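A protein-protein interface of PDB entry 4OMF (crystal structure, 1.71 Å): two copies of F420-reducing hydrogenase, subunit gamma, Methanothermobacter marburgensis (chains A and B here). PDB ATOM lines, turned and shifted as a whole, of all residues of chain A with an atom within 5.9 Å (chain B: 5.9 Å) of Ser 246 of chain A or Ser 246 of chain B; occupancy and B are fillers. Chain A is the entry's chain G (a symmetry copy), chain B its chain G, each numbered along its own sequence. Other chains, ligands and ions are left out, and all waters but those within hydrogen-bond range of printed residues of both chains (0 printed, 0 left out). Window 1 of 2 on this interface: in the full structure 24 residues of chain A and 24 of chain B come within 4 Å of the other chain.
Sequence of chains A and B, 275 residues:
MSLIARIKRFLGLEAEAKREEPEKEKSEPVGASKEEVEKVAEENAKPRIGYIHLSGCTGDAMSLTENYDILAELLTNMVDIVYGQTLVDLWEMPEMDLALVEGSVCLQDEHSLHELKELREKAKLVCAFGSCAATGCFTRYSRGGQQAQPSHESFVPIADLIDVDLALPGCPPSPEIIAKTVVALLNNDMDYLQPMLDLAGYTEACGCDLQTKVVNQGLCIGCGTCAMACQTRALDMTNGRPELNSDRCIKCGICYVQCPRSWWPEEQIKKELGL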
ATOM      1  N   TYR A 141       7.797  37.458 -15.842  1.00  0.00           N
ATOM      2  CA  TYR A 141       7.326  37.680 -17.222  1.00  0.00           C
ATOM      3  C   TYR A 141       7.555  39.099 -17.779  1.00  0.00           C
ATOM      4  O   TYR A 141       7.359  39.342 -18.985  1.00  0.00           O
ATOM      5  CB  TYR A 141       5.824  37.362 -17.337  1.00  0.00           C
ATOM      6  CG  TYR A 141       5.479  35.939 -17.002  1.00  0.00           C
ATOM      7  CD1 TYR A 141       5.997  34.882 -17.741  1.00  0.00           C
ATOM      8  CD2 TYR A 141       4.612  35.641 -15.957  1.00  0.00           C
ATOM      9  CE1 TYR A 141       5.658  33.558 -17.436  1.00  0.00           C
ATOM     10  CE2 TYR A 141       4.284  34.321 -15.651  1.00  0.00           C
ATOM     11  CZ  TYR A 141       4.810  33.299 -16.395  1.00  0.00           C
ATOM     12  OH  TYR A 141       4.473  32.002 -16.084  1.00  0.00           O
ATOM     13  N   CYS A 208       6.223  23.719 -13.121  1.00  0.00           N
ATOM     14  CA  CYS A 208       6.978  22.569 -13.639  1.00  0.00           C
ATOM     15  C   CYS A 208       7.876  21.959 -12.563  1.00  0.00           C
ATOM     16  O   CYS A 208       8.346  20.829 -12.726  1.00  0.00           O
ATOM     17  CB  CYS A 208       7.853  22.976 -14.833  1.00  0.00           C
ATOM     18  SG  CYS A 208       6.995  23.529 -16.320  1.00  0.00           S
ATOM     19  N   ALA A 234      -4.081  27.243 -11.525  1.00  0.00           N
ATOM     20  CA  ALA A 234      -3.327  26.780 -12.706  1.00  0.00           C
ATOM     21  C   ALA A 234      -3.233  25.266 -12.729  1.00  0.00           C
ATOM     22  O   ALA A 234      -2.865  24.684 -13.747  1.00  0.00           O
ATOM     23  CB  ALA A 234      -1.921  27.361 -12.732  1.00  0.00           C
ATOM     24  N   LEU A 244      -0.595  21.065 -15.321  1.00  0.00           N
ATOM     25  CA  LEU A 244      -0.335  22.514 -15.260  1.00  0.00           C
ATOM     26  C   LEU A 244      -0.948  23.279 -16.438  1.00  0.00           C
ATOM     27  O   LEU A 244      -0.723  22.914 -17.592  1.00  0.00           O
ATOM     28  CB  LEU A 244       1.176  22.756 -15.230  1.00  0.00           C
ATOM     29  CG  LEU A 244       1.648  24.218 -15.237  1.00  0.00           C
ATOM     30  CD1 LEU A 244       1.152  24.943 -13.965  1.00  0.00           C
ATOM     31  CD2 LEU A 244       3.164  24.281 -15.322  1.00  0.00           C
ATOM     32  N   ASN A 245      -1.741  24.313 -16.137  1.00  0.00           N
ATOM     33  CA  ASN A 245      -2.211  25.248 -17.166  1.00  0.00           C
ATOM     34  C   ASN A 245      -1.236  26.403 -17.143  1.00  0.00           C
ATOM     35  O   ASN A 245      -1.334  27.290 -16.295  1.00  0.00           O
ATOM     36  CB  ASN A 245      -3.661  25.705 -16.904  1.00  0.00           C
ATOM     37  CG  ASN A 245      -4.131  26.786 -17.883  1.00  0.00           C
ATOM     38  OD1 ASN A 245      -3.370  27.248 -18.747  1.00  0.00           O
ATOM     39  ND2 ASN A 245      -5.403  27.170 -17.771  1.00  0.00           N
ATOM     40  N   SER A 246      -0.254  26.377 -18.045  1.00  0.00           N
ATOM     41  CA  SER A 246       0.818  27.371 -18.016  1.00  0.00           C
ATOM     42  C   SER A 246       0.333  28.808 -18.210  1.00  0.00           C
ATOM     43  O   SER A 246       0.999  29.760 -17.785  1.00  0.00           O
ATOM     44  CB  SER A 246       1.873  27.043 -19.074  1.00  0.00           C
ATOM     45  OG  SER A 246       2.787  26.099 -18.560  1.00  0.00           O
ATOM     46  N   ASP A 247      -0.820  28.958 -18.839  1.00  0.00           N
ATOM     47  CA  ASP A 247      -1.399  30.286 -19.072  1.00  0.00           C
ATOM     48  C   ASP A 247      -1.795  30.981 -17.772  1.00  0.00           C
ATOM     49  O   ASP A 247      -1.971  32.207 -17.754  1.00  0.00           O
ATOM     50  CB  ASP A 247      -2.625  30.203 -19.976  1.00  0.00           C
ATOM     51  CG  ASP A 247      -2.282  29.771 -21.408  1.00  0.00           C
ATOM     52  OD1 ASP A 247      -1.100  29.845 -21.805  1.00  0.00           O
ATOM     53  OD2 ASP A 247      -3.214  29.394 -22.135  1.00  0.00           O
ATOM     54  N   ARG A 248      -1.915  30.217 -16.688  1.00  0.00           N
ATOM     55  CA  ARG A 248      -2.318  30.789 -15.390  1.00  0.00           C
ATOM     56  C   ARG A 248      -1.206  30.755 -14.344  1.00  0.00           C
ATOM     57  O   ARG A 248      -1.409  31.218 -13.205  1.00  0.00           O
ATOM     58  CB  ARG A 248      -3.558  30.059 -14.827  1.00  0.00           C
ATOM     59  CG  ARG A 248      -4.804  30.081 -15.753  1.00  0.00           C
ATOM     60  CD  ARG A 248      -6.017  29.401 -15.100  1.00  0.00           C
ATOM     61  NE  ARG A 248      -6.460  30.239 -13.988  1.00  0.00           N
ATOM     62  CZ  ARG A 248      -7.288  31.266 -14.111  1.00  0.00           C
ATOM     63  NH1 ARG A 248      -7.583  32.001 -13.046  1.00  0.00           N
ATOM     64  NH2 ARG A 248      -7.816  31.571 -15.298  1.00  0.00           N
ATOM     65  N   CYS A 249      -0.032  30.233 -14.708  1.00  0.00           N
ATOM     66  CA  CYS A 249       1.044  30.079 -13.704  1.00  0.00           C
ATOM     67  C   CYS A 249       1.771  31.390 -13.480  1.00  0.00           C
ATOM     68  O   CYS A 249       2.226  32.014 -14.450  1.00  0.00           O
ATOM     69  CB  CYS A 249       2.062  29.009 -14.122  1.00  0.00           C
ATOM     70  SG  CYS A 249       3.300  28.692 -12.807  1.00  0.00           S
ATOM     71  N   TYR B 141       8.037  15.713 -18.880  1.00  0.00           N
ATOM     72  CA  TYR B 141       6.566  15.651 -18.791  1.00  0.00           C
ATOM     73  C   TYR B 141       5.981  14.261 -18.471  1.00  0.00           C
ATOM     74  O   TYR B 141       4.772  14.133 -18.200  1.00  0.00           O
ATOM     75  CB  TYR B 141       5.925  16.144 -20.102  1.00  0.00           C
ATOM     76  CG  TYR B 141       6.262  17.568 -20.442  1.00  0.00           C
ATOM     77  CD1 TYR B 141       5.901  18.611 -19.600  1.00  0.00           C
ATOM     78  CD2 TYR B 141       6.927  17.882 -21.623  1.00  0.00           C
ATOM     79  CE1 TYR B 141       6.202  19.938 -19.930  1.00  0.00           C
ATOM     80  CE2 TYR B 141       7.232  19.204 -21.943  1.00  0.00           C
ATOM     81  CZ  TYR B 141       6.865  20.213 -21.094  1.00  0.00           C
ATOM     82  OH  TYR B 141       7.168  21.512 -21.427  1.00  0.00           O
ATOM     83  N   CYS B 208      11.490  29.298 -20.350  1.00  0.00           N
ATOM     84  CA  CYS B 208      11.432  30.392 -19.370  1.00  0.00           C
ATOM     85  C   CYS B 208      12.829  30.813 -18.918  1.00  0.00           C
ATOM     86  O   CYS B 208      12.986  31.892 -18.338  1.00  0.00           O
ATOM     87  CB  CYS B 208      10.621  29.979 -18.132  1.00  0.00           C
ATOM     88  SG  CYS B 208       8.868  29.639 -18.383  1.00  0.00           S
ATOM     89  N   ALA B 234       8.642  26.852 -30.696  1.00  0.00           N
ATOM     90  CA  ALA B 234       7.897  27.314 -29.510  1.00  0.00           C
ATOM     91  C   ALA B 234       8.083  28.805 -29.301  1.00  0.00           C
ATOM     92  O   ALA B 234       7.354  29.417 -28.523  1.00  0.00           O
ATOM     93  CB  ALA B 234       8.341  26.582 -28.253  1.00  0.00           C
ATOM     94  N   LEU B 244       7.180  32.864 -25.554  1.00  0.00           N
ATOM     95  CA  LEU B 244       7.171  31.395 -25.448  1.00  0.00           C
ATOM     96  C   LEU B 244       5.770  30.794 -25.611  1.00  0.00           C
ATOM     97  O   LEU B 244       4.838  31.217 -24.928  1.00  0.00           O
ATOM     98  CB  LEU B 244       7.745  30.981 -24.091  1.00  0.00           C
ATOM     99  CG  LEU B 244       7.753  29.480 -23.765  1.00  0.00           C
ATOM    100  CD1 LEU B 244       8.650  28.722 -24.770  1.00  0.00           C
ATOM    101  CD2 LEU B 244       8.243  29.253 -22.345  1.00  0.00           C
ATOM    102  N   ASN B 245       5.629  29.837 -26.533  1.00  0.00           N
ATOM    103  CA  ASN B 245       4.400  29.041 -26.635  1.00  0.00           C
ATOM    104  C   ASN B 245       4.661  27.785 -25.835  1.00  0.00           C
ATOM    105  O   ASN B 245       5.302  26.853 -26.322  1.00  0.00           O
ATOM    106  CB  ASN B 245       4.037  28.733 -28.102  1.00  0.00           C
ATOM    107  CG  ASN B 245       2.838  27.788 -28.234  1.00  0.00           C
ATOM    108  OD1 ASN B 245       2.281  27.310 -27.234  1.00  0.00           O
ATOM    109  ND2 ASN B 245       2.414  27.543 -29.474  1.00  0.00           N
ATOM    110  N   SER B 246       4.208  27.767 -24.580  1.00  0.00           N
ATOM    111  CA  SER B 246       4.530  26.659 -23.682  1.00  0.00           C
ATOM    112  C   SER B 246       4.005  25.305 -24.161  1.00  0.00           C
ATOM    113  O   SER B 246       4.540  24.255 -23.786  1.00  0.00           O
ATOM    114  CB  SER B 246       3.997  26.944 -22.277  1.00  0.00           C
ATOM    115  OG  SER B 246       4.922  27.738 -21.567  1.00  0.00           O
ATOM    116  N   ASP B 247       2.972  25.334 -24.985  1.00  0.00           N
ATOM    117  CA  ASP B 247       2.388  24.101 -25.526  1.00  0.00           C
ATOM    118  C   ASP B 247       3.353  23.359 -26.448  1.00  0.00           C
ATOM    119  O   ASP B 247       3.164  22.164 -26.708  1.00  0.00           O
ATOM    120  CB  ASP B 247       1.102  24.390 -26.293  1.00  0.00           C
ATOM    121  CG  ASP B 247      -0.033  24.887 -25.389  1.00  0.00           C
ATOM    122  OD1 ASP B 247       0.043  24.710 -24.155  1.00  0.00           O
ATOM    123  OD2 ASP B 247      -1.013  25.421 -25.934  1.00  0.00           O
ATOM    124  N   ARG B 248       4.389  24.048 -26.922  1.00  0.00           N
ATOM    125  CA  ARG B 248       5.362  23.430 -27.841  1.00  0.00           C
ATOM    126  C   ARG B 248       6.750  23.259 -27.224  1.00  0.00           C
ATOM    127  O   ARG B 248       7.666  22.738 -27.889  1.00  0.00           O
ATOM    128  CB  ARG B 248       5.491  24.251 -29.143  1.00  0.00           C
ATOM    129  CG  ARG B 248       4.165  24.439 -29.928  1.00  0.00           C
ATOM    130  CD  ARG B 248       4.381  25.201 -31.245  1.00  0.00           C
ATOM    131  NE  ARG B 248       5.139  24.338 -32.148  1.00  0.00           N
ATOM    132  CZ  ARG B 248       4.596  23.422 -32.937  1.00  0.00           C
ATOM    133  NH1 ARG B 248       5.377  22.648 -33.677  1.00  0.00           N
ATOM    134  NH2 ARG B 248       3.270  23.270 -32.983  1.00  0.00           N
ATOM    135  N   CYS B 249       6.920  23.671 -25.965  1.00  0.00           N
ATOM    136  CA  CYS B 249       8.269  23.627 -25.357  1.00  0.00           C
ATOM    137  C   CYS B 249       8.601  22.228 -24.875  1.00  0.00           C
ATOM    138  O   CYS B 249       7.814  21.632 -24.126  1.00  0.00           O
ATOM    139  CB  CYS B 249       8.392  24.602 -24.179  1.00  0.00           C
ATOM    140  SG  CYS B 249      10.105  24.679 -23.530  1.00  0.00           S
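Ser 246 of chain A touches Ser 246 of chain B (CB to CB, 3.8 Å).
Of the printed residues of chain B, Ser 246 of chain A touches Ser 246 (3.8 Å). Leu 244 of chain B touches none of the printed residues of chain A. Printed residues of chain A within 4 Å of Ser 246 of chain B: Ser 246 (3.8 Å). The nearest printed residue of chain A that does not touch Ser 246 of chain B is Asp 247 of chain A (5.9 Å).
Of the 9 printed residues of chain A, 1 touches a printed residue of chain B. Printed residues of chain A that touch a printed residue of chain B: Ser 246. Of the 9 printed residues of chain B, 1 touches a printed residue of chain A. Among the printed residues, 1 pair touches across the chains. Among the printed residues, no Asp or Glu carboxylate lies within 4 Å of a Lys or Arg side-chain nitrogen of the other chain.
Ser 246 of chain B touches its own counterpart, Ser 246 of chain A.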
